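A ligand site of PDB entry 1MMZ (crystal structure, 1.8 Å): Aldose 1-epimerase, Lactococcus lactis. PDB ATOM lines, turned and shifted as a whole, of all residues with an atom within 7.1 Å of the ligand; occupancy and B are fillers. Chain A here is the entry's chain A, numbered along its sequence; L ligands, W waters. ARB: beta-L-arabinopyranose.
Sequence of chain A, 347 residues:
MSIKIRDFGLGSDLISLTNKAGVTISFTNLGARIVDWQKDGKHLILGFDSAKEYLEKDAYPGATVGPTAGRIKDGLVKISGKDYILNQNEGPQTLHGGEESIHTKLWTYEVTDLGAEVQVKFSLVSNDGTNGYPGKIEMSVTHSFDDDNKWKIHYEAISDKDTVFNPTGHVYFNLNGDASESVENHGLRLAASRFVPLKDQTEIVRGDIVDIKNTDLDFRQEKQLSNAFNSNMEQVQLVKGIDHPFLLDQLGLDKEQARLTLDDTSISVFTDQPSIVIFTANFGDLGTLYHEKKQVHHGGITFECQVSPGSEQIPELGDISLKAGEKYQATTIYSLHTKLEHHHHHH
OD1 of Asp 243 sits at hydrogen-bond distance from O2 of the ligand, at 2.5 Å.
The side-chain carboxylate (OE2) of Glu 304 sits at hydrogen-bond distance from an oxygen (O1) of the ligand (2.6 Å).
NE2 of His 170 is in hydrogen-bond range of O5 of the ligand (2.7 Å).
NE2 of His 96 sits at hydrogen-bond distance from O5 of the ligand, 3.1 Å away.
O3 of the ligand is in hydrogen-bond range of NH2 of Arg 71 (3.1 Å).
N of Asp 243 sits close to O of Ile 278.
The side-chain carboxylate of Glu 304 lies within hydrogen-bond range of the side-chain hydroxyl of Thr 302 (2.8 Å).
The backbone NH of Val 277 sits at hydrogen-bond distance from the backbone carbonyl oxygen of Glu 304 (2.9 Å).
O of Phe 279 is in hydrogen-bond range of N of Thr 302.
The backbone NH of His 96 lies within hydrogen-bond range of the backbone carbonyl oxygen of Gly 70 (2.9 Å).
The guanidinium group (NH2) of Arg 71 is in salt-bridge range of the side-chain carboxylate (OE1) of Glu 203, 3.7 Å away.
The guanidinium group (NE) of Arg 71 is in salt-bridge range of the side-chain carboxylate (OE1) of Glu 90, at 2.8 Å.
Tyr 172 touches the ligand (OH to C5, 3.998 Å).
Glu 203 touches the ligand.
CB of Phe 279 touches O1 of the ligand, 3.1 Å away.
Eight residues have an atom within 4 Å of the ligand: Arg 71, His 96, His 170, Tyr 172, Glu 203, Asp 243, Phe 279 and Glu 304.
The nearest printed residue that does not touch the ligand is Thr 302 (4.5 Å).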
ATOM      1  N   ASP A  58       6.613  10.135 -17.581  1.00  0.00           N
ATOM      2  CA  ASP A  58       5.763  11.215 -17.988  1.00  0.00           C
ATOM      3  C   ASP A  58       5.633  11.055 -19.470  1.00  0.00           C
ATOM      4  O   ASP A  58       6.646  11.079 -20.155  1.00  0.00           O
ATOM      5  CB  ASP A  58       6.329  12.608 -17.598  1.00  0.00           C
ATOM      6  CG  ASP A  58       5.466  13.772 -18.074  1.00  0.00           C
ATOM      7  OD1 ASP A  58       4.443  13.669 -18.716  1.00  0.00           O
ATOM      8  OD2 ASP A  58       5.950  14.927 -17.758  1.00  0.00           O
ATOM      9  N   TYR A  60       3.990  12.988 -21.537  1.00  0.00           N
ATOM     10  CA  TYR A  60       3.772  14.202 -22.302  1.00  0.00           C
ATOM     11  C   TYR A  60       4.914  14.842 -23.039  1.00  0.00           C
ATOM     12  O   TYR A  60       4.690  15.380 -24.132  1.00  0.00           O
ATOM     13  CB  TYR A  60       3.121  15.276 -21.459  1.00  0.00           C
ATOM     14  CG  TYR A  60       1.673  14.888 -21.135  1.00  0.00           C
ATOM     15  CD1 TYR A  60       1.274  14.709 -19.819  1.00  0.00           C
ATOM     16  CD2 TYR A  60       0.734  14.689 -22.147  1.00  0.00           C
ATOM     17  CE1 TYR A  60      -0.032  14.349 -19.479  1.00  0.00           C
ATOM     18  CE2 TYR A  60      -0.586  14.338 -21.825  1.00  0.00           C
ATOM     19  CZ  TYR A  60      -0.971  14.174 -20.495  1.00  0.00           C
ATOM     20  OH  TYR A  60      -2.259  13.823 -20.153  1.00  0.00           O
ATOM     21  N   VAL A  65      -0.156  16.089 -28.612  1.00  0.00           N
ATOM     22  CA  VAL A  65      -1.264  15.880 -27.665  1.00  0.00           C
ATOM     23  C   VAL A  65      -2.537  16.349 -28.323  1.00  0.00           C
ATOM     24  O   VAL A  65      -2.509  17.288 -29.094  1.00  0.00           O
ATOM     25  CB  VAL A  65      -1.209  16.583 -26.293  1.00  0.00           C
ATOM     26  CG1 VAL A  65      -0.033  16.121 -25.434  1.00  0.00           C
ATOM     27  CG2 VAL A  65      -1.193  18.080 -26.476  1.00  0.00           C
ATOM     28  N   GLY A  70      -4.749  21.002 -23.825  1.00  0.00           N
ATOM     29  CA  GLY A  70      -5.140  21.840 -22.719  1.00  0.00           C
ATOM     30  C   GLY A  70      -6.301  21.288 -21.916  1.00  0.00           C
ATOM     31  O   GLY A  70      -6.708  20.154 -22.115  1.00  0.00           O
ATOM     32  N   ARG A  71      -6.823  22.118 -20.997  1.00  0.00           N
ATOM     33  CA  ARG A  71      -7.935  21.739 -20.127  1.00  0.00           C
ATOM     34  C   ARG A  71      -9.270  22.242 -20.610  1.00  0.00           C
ATOM     35  O   ARG A  71      -9.403  23.449 -20.932  1.00  0.00           O
ATOM     36  CB  ARG A  71      -7.773  22.413 -18.775  1.00  0.00           C
ATOM     37  CG  ARG A  71      -6.594  21.808 -18.069  1.00  0.00           C
ATOM     38  CD  ARG A  71      -6.287  22.445 -16.720  1.00  0.00           C
ATOM     39  NE  ARG A  71      -5.180  21.681 -16.138  1.00  0.00           N
ATOM     40  CZ  ARG A  71      -3.878  21.878 -16.408  1.00  0.00           C
ATOM     41  NH1 ARG A  71      -3.410  22.890 -17.198  1.00  0.00           N
ATOM     42  NH2 ARG A  71      -3.042  21.045 -15.820  1.00  0.00           N
ATOM     43  N   GLU A  90      -8.630  14.653 -15.110  1.00  0.00           N
ATOM     44  CA  GLU A  90      -7.972  15.542 -14.174  1.00  0.00           C
ATOM     45  C   GLU A  90      -9.098  16.178 -13.422  1.00  0.00           C
ATOM     46  O   GLU A  90      -9.573  17.300 -13.740  1.00  0.00           O
ATOM     47  CB  GLU A  90      -7.219  16.623 -14.899  1.00  0.00           C
ATOM     48  CG  GLU A  90      -6.240  17.258 -13.934  1.00  0.00           C
ATOM     49  CD  GLU A  90      -5.693  18.555 -14.451  1.00  0.00           C
ATOM     50  OE1 GLU A  90      -6.373  19.461 -14.867  1.00  0.00           O
ATOM     51  OE2 GLU A  90      -4.402  18.627 -14.382  1.00  0.00           O
ATOM     52  N   LEU A  95      -8.145  16.874 -19.738  1.00  0.00           N
ATOM     53  CA  LEU A  95      -6.859  17.494 -19.996  1.00  0.00           C
ATOM     54  C   LEU A  95      -6.119  16.772 -21.117  1.00  0.00           C
ATOM     55  O   LEU A  95      -5.954  15.574 -21.094  1.00  0.00           O
ATOM     56  CB  LEU A  95      -5.996  17.466 -18.702  1.00  0.00           C
ATOM     57  CG  LEU A  95      -4.492  17.629 -18.995  1.00  0.00           C
ATOM     58  CD1 LEU A  95      -4.162  19.130 -19.162  1.00  0.00           C
ATOM     59  CD2 LEU A  95      -3.703  17.056 -17.838  1.00  0.00           C
ATOM     60  N   HIS A  96      -5.667  17.489 -22.102  1.00  0.00           N
ATOM     61  CA  HIS A  96      -4.933  16.862 -23.197  1.00  0.00           C
ATOM     62  C   HIS A  96      -5.625  15.676 -23.902  1.00  0.00           C
ATOM     63  O   HIS A  96      -4.972  14.668 -24.219  1.00  0.00           O
ATOM     64  CB  HIS A  96      -3.504  16.475 -22.778  1.00  0.00           C
ATOM     65  CG  HIS A  96      -2.699  17.670 -22.384  1.00  0.00           C
ATOM     66  ND1 HIS A  96      -2.889  18.906 -23.008  1.00  0.00           N
ATOM     67  CD2 HIS A  96      -1.732  17.791 -21.456  1.00  0.00           C
ATOM     68  CE1 HIS A  96      -2.050  19.750 -22.431  1.00  0.00           C
ATOM     69  NE2 HIS A  96      -1.320  19.106 -21.510  1.00  0.00           N
ATOM     70  N   HIS A 170       4.181  19.109 -27.503  1.00  0.00           N
ATOM     71  CA  HIS A 170       4.576  19.355 -26.137  1.00  0.00           C
ATOM     72  C   HIS A 170       6.081  19.235 -25.802  1.00  0.00           C
ATOM     73  O   HIS A 170       6.431  18.784 -24.728  1.00  0.00           O
ATOM     74  CB  HIS A 170       3.722  18.411 -25.260  1.00  0.00           C
ATOM     75  CG  HIS A 170       3.388  18.945 -23.885  1.00  0.00           C
ATOM     76  ND1 HIS A 170       4.370  19.041 -22.881  1.00  0.00           N
ATOM     77  CD2 HIS A 170       2.203  19.361 -23.388  1.00  0.00           C
ATOM     78  CE1 HIS A 170       3.748  19.526 -21.816  1.00  0.00           C
ATOM     79  NE2 HIS A 170       2.459  19.734 -22.078  1.00  0.00           N
ATOM     80  N   TYR A 172       9.672  20.198 -24.421  1.00  0.00           N
ATOM     81  CA  TYR A 172      10.167  21.042 -23.350  1.00  0.00           C
ATOM     82  C   TYR A 172      11.616  21.399 -23.734  1.00  0.00           C
ATOM     83  O   TYR A 172      12.444  20.528 -24.027  1.00  0.00           O
ATOM     84  CB  TYR A 172      10.308  20.336 -21.990  1.00  0.00           C
ATOM     85  CG  TYR A 172       9.021  20.096 -21.203  1.00  0.00           C
ATOM     86  CD1 TYR A 172       8.298  18.915 -21.398  1.00  0.00           C
ATOM     87  CD2 TYR A 172       8.574  20.986 -20.228  1.00  0.00           C
ATOM     88  CE1 TYR A 172       7.149  18.659 -20.660  1.00  0.00           C
ATOM     89  CE2 TYR A 172       7.425  20.750 -19.474  1.00  0.00           C
ATOM     90  CZ  TYR A 172       6.715  19.572 -19.699  1.00  0.00           C
ATOM     91  OH  TYR A 172       5.575  19.318 -18.950  1.00  0.00           O
ATOM     92  N   LEU A 198      -5.724  32.197 -14.997  1.00  0.00           N
ATOM     93  CA  LEU A 198      -6.333  30.989 -14.538  1.00  0.00           C
ATOM     94  C   LEU A 198      -7.250  31.225 -13.338  1.00  0.00           C
ATOM     95  O   LEU A 198      -6.990  32.075 -12.500  1.00  0.00           O
ATOM     96  CB  LEU A 198      -5.225  29.960 -14.226  1.00  0.00           C
ATOM     97  CG  LEU A 198      -4.264  29.757 -15.376  1.00  0.00           C
ATOM     98  CD1 LEU A 198      -3.278  28.643 -15.002  1.00  0.00           C
ATOM     99  CD2 LEU A 198      -5.021  29.381 -16.657  1.00  0.00           C
ATOM    100  N   GLU A 203      -6.626  25.214 -12.591  1.00  0.00           N
ATOM    101  CA  GLU A 203      -6.096  25.672 -13.844  1.00  0.00           C
ATOM    102  C   GLU A 203      -7.083  25.855 -14.969  1.00  0.00           C
ATOM    103  O   GLU A 203      -6.685  25.929 -16.117  1.00  0.00           O
ATOM    104  CB  GLU A 203      -4.859  24.873 -14.259  1.00  0.00           C
ATOM    105  CG  GLU A 203      -3.625  25.187 -13.366  1.00  0.00           C
ATOM    106  CD  GLU A 203      -2.598  24.084 -13.197  1.00  0.00           C
ATOM    107  OE1 GLU A 203      -2.865  22.979 -12.726  1.00  0.00           O
ATOM    108  OE2 GLU A 203      -1.381  24.453 -13.492  1.00  0.00           O
ATOM    109  N   ILE A 242       5.086  29.884 -14.707  1.00  0.00           N
ATOM    110  CA  ILE A 242       4.152  30.253 -15.762  1.00  0.00           C
ATOM    111  C   ILE A 242       3.479  28.972 -16.213  1.00  0.00           C
ATOM    112  O   ILE A 242       4.106  27.914 -16.201  1.00  0.00           O
ATOM    113  CB  ILE A 242       4.863  30.937 -16.956  1.00  0.00           C
ATOM    114  CG1 ILE A 242       5.816  32.011 -16.432  1.00  0.00           C
ATOM    115  CG2 ILE A 242       3.883  31.525 -18.002  1.00  0.00           C
ATOM    116  CD1 ILE A 242       6.669  32.613 -17.516  1.00  0.00           C
ATOM    117  N   ASP A 243       2.207  29.073 -16.526  1.00  0.00           N
ATOM    118  CA  ASP A 243       1.403  27.964 -17.011  1.00  0.00           C
ATOM    119  C   ASP A 243       0.188  28.614 -17.610  1.00  0.00           C
ATOM    120  O   ASP A 243      -0.893  28.417 -17.116  1.00  0.00           O
ATOM    121  CB  ASP A 243       1.041  26.937 -15.916  1.00  0.00           C
ATOM    122  CG  ASP A 243       0.500  25.685 -16.548  1.00  0.00           C
ATOM    123  OD1 ASP A 243       0.345  25.550 -17.753  1.00  0.00           O
ATOM    124  OD2 ASP A 243       0.254  24.734 -15.703  1.00  0.00           O
ATOM    125  N   HIS A 244       0.404  29.432 -18.667  1.00  0.00           N
ATOM    126  CA  HIS A 244      -0.619  30.234 -19.260  1.00  0.00           C
ATOM    127  C   HIS A 244      -0.553  30.415 -20.735  1.00  0.00           C
ATOM    128  O   HIS A 244       0.529  30.396 -21.340  1.00  0.00           O
ATOM    129  CB  HIS A 244      -0.388  31.676 -18.746  1.00  0.00           C
ATOM    130  CG  HIS A 244      -0.588  31.794 -17.260  1.00  0.00           C
ATOM    131  ND1 HIS A 244       0.385  31.402 -16.337  1.00  0.00           N
ATOM    132  CD2 HIS A 244      -1.669  32.254 -16.587  1.00  0.00           C
ATOM    133  CE1 HIS A 244      -0.119  31.583 -15.128  1.00  0.00           C
ATOM    134  NE2 HIS A 244      -1.344  32.116 -15.252  1.00  0.00           N
ATOM    135  N   VAL A 277       0.860  28.538 -25.375  1.00  0.00           N
ATOM    136  CA  VAL A 277       0.752  28.241 -23.993  1.00  0.00           C
ATOM    137  C   VAL A 277       2.156  27.987 -23.465  1.00  0.00           C
ATOM    138  O   VAL A 277       2.901  27.157 -23.984  1.00  0.00           O
ATOM    139  CB  VAL A 277      -0.131  27.027 -23.759  1.00  0.00           C
ATOM    140  CG1 VAL A 277       0.034  26.601 -22.302  1.00  0.00           C
ATOM    141  CG2 VAL A 277      -1.590  27.406 -24.003  1.00  0.00           C
ATOM    142  N   ILE A 278       2.544  28.669 -22.405  1.00  0.00           N
ATOM    143  CA  ILE A 278       3.874  28.472 -21.891  1.00  0.00           C
ATOM    144  C   ILE A 278       3.857  27.837 -20.550  1.00  0.00           C
ATOM    145  O   ILE A 278       3.232  28.364 -19.639  1.00  0.00           O
ATOM    146  CB  ILE A 278       4.596  29.811 -21.798  1.00  0.00           C
ATOM    147  CG1 ILE A 278       4.741  30.348 -23.209  1.00  0.00           C
ATOM    148  CG2 ILE A 278       5.962  29.698 -21.096  1.00  0.00           C
ATOM    149  CD1 ILE A 278       5.581  31.600 -23.246  1.00  0.00           C
ATOM    150  N   PHE A 279       4.527  26.709 -20.413  1.00  0.00           N
ATOM    151  CA  PHE A 279       4.568  26.055 -19.099  1.00  0.00           C
ATOM    152  C   PHE A 279       6.028  25.838 -18.717  1.00  0.00           C
ATOM    153  O   PHE A 279       6.810  25.308 -19.518  1.00  0.00           O
ATOM    154  CB  PHE A 279       3.733  24.765 -19.125  1.00  0.00           C
ATOM    155  CG  PHE A 279       3.960  23.835 -17.972  1.00  0.00           C
ATOM    156  CD1 PHE A 279       3.541  24.183 -16.688  1.00  0.00           C
ATOM    157  CD2 PHE A 279       4.554  22.588 -18.187  1.00  0.00           C
ATOM    158  CE1 PHE A 279       3.702  23.329 -15.597  1.00  0.00           C
ATOM    159  CE2 PHE A 279       4.738  21.716 -17.112  1.00  0.00           C
ATOM    160  CZ  PHE A 279       4.301  22.079 -15.834  1.00  0.00           C
ATOM    161  N   THR A 280       6.392  26.297 -17.541  1.00  0.00           N
ATOM    162  CA  THR A 280       7.785  26.228 -17.066  1.00  0.00           C
ATOM    163  C   THR A 280       8.137  25.104 -16.104  1.00  0.00           C
ATOM    164  O   THR A 280       8.900  25.302 -15.140  1.00  0.00           O
ATOM    165  CB  THR A 280       8.212  27.577 -16.458  1.00  0.00           C
ATOM    166  OG1 THR A 280       7.284  27.949 -15.469  1.00  0.00           O
ATOM    167  CG2 THR A 280       8.228  28.632 -17.539  1.00  0.00           C
ATOM    168  N   ASN A 282       6.811  23.538 -13.573  1.00  0.00           N
ATOM    169  CA  ASN A 282       6.662  23.884 -12.170  1.00  0.00           C
ATOM    170  C   ASN A 282       6.398  22.675 -11.282  1.00  0.00           C
ATOM    171  O   ASN A 282       5.448  22.657 -10.493  1.00  0.00           O
ATOM    172  CB  ASN A 282       5.518  24.925 -12.054  1.00  0.00           C
ATOM    173  CG  ASN A 282       5.582  26.036 -13.110  1.00  0.00           C
ATOM    174  OD1 ASN A 282       6.675  26.471 -13.508  1.00  0.00           O
ATOM    175  ND2 ASN A 282       4.419  26.486 -13.568  1.00  0.00           N
ATOM    176  N   PHE A 283       7.241  21.645 -11.401  1.00  0.00           N
ATOM    177  CA  PHE A 283       7.049  20.391 -10.630  1.00  0.00           C
ATOM    178  C   PHE A 283       7.552  20.322  -9.186  1.00  0.00           C
ATOM    179  O   PHE A 283       7.491  19.277  -8.526  1.00  0.00           O
ATOM    180  CB  PHE A 283       7.561  19.177 -11.415  1.00  0.00           C
ATOM    181  CG  PHE A 283       7.044  19.095 -12.849  1.00  0.00           C
ATOM    182  CD1 PHE A 283       7.887  19.306 -13.946  1.00  0.00           C
ATOM    183  CD2 PHE A 283       5.709  18.779 -13.098  1.00  0.00           C
ATOM    184  CE1 PHE A 283       7.421  19.206 -15.261  1.00  0.00           C
ATOM    185  CE2 PHE A 283       5.216  18.685 -14.400  1.00  0.00           C
ATOM    186  CZ  PHE A 283       6.081  18.891 -15.479  1.00  0.00           C
ATOM    187  N   THR A 302       7.827  25.022 -22.143  1.00  0.00           N
ATOM    188  CA  THR A 302       7.174  24.637 -23.397  1.00  0.00           C
ATOM    189  C   THR A 302       6.746  25.823 -24.186  1.00  0.00           C
ATOM    190  O   THR A 302       6.612  26.889 -23.635  1.00  0.00           O
ATOM    191  CB  THR A 302       5.862  23.861 -23.098  1.00  0.00           C
ATOM    192  OG1 THR A 302       4.991  24.752 -22.457  1.00  0.00           O
ATOM    193  CG2 THR A 302       6.072  22.647 -22.178  1.00  0.00           C
ATOM    194  N   GLU A 304       3.620  25.664 -26.465  1.00  0.00           N
ATOM    195  CA  GLU A 304       2.505  24.913 -27.034  1.00  0.00           C
ATOM    196  C   GLU A 304       1.678  25.802 -27.928  1.00  0.00           C
ATOM    197  O   GLU A 304       0.872  26.568 -27.467  1.00  0.00           O
ATOM    198  CB  GLU A 304       1.639  24.280 -25.906  1.00  0.00           C
ATOM    199  CG  GLU A 304       2.494  23.343 -25.036  1.00  0.00           C
ATOM    200  CD  GLU A 304       1.882  22.981 -23.703  1.00  0.00           C
ATOM    201  OE1 GLU A 304       0.797  22.490 -23.590  1.00  0.00           O
ATOM    202  OE2 GLU A 304       2.636  23.248 -22.669  1.00  0.00           O
ATOM    203  N   PRO A 309      -6.625  27.506 -24.769  1.00  0.00           N
ATOM    204  CA  PRO A 309      -7.620  26.742 -24.057  1.00  0.00           C
ATOM    205  C   PRO A 309      -8.624  27.742 -23.436  1.00  0.00           C
ATOM    206  O   PRO A 309      -8.322  28.915 -23.288  1.00  0.00           O
ATOM    207  CB  PRO A 309      -6.890  26.020 -22.899  1.00  0.00           C
ATOM    208  CG  PRO A 309      -5.407  26.360 -23.029  1.00  0.00           C
ATOM    209  CD  PRO A 309      -5.248  27.259 -24.238  1.00  0.00           C
HETATM  210  C1  ARB L   1       0.538  21.916 -20.103  1.00  0.00           C
HETATM  211  C2  ARB L   1      -0.325  22.307 -18.883  1.00  0.00           C
HETATM  212  C3  ARB L   1       0.475  22.123 -17.620  1.00  0.00           C
HETATM  213  C4  ARB L   1       0.926  20.683 -17.512  1.00  0.00           C
HETATM  214  C5  ARB L   1       1.684  20.221 -18.771  1.00  0.00           C
HETATM  215  O1  ARB L   1       1.647  22.789 -20.269  1.00  0.00           O
HETATM  216  O2  ARB L   1      -0.805  23.676 -18.917  1.00  0.00           O
HETATM  217  O3  ARB L   1      -0.315  22.434 -16.475  1.00  0.00           O
HETATM  218  O4  ARB L   1      -0.109  19.780 -17.180  1.00  0.00           O
HETATM  219  O5  ARB L   1       0.987  20.548 -20.007  1.00  0.00           O
HETATM  220  O   HOH W   1      -2.695  24.068 -21.223  1.00  0.00           O
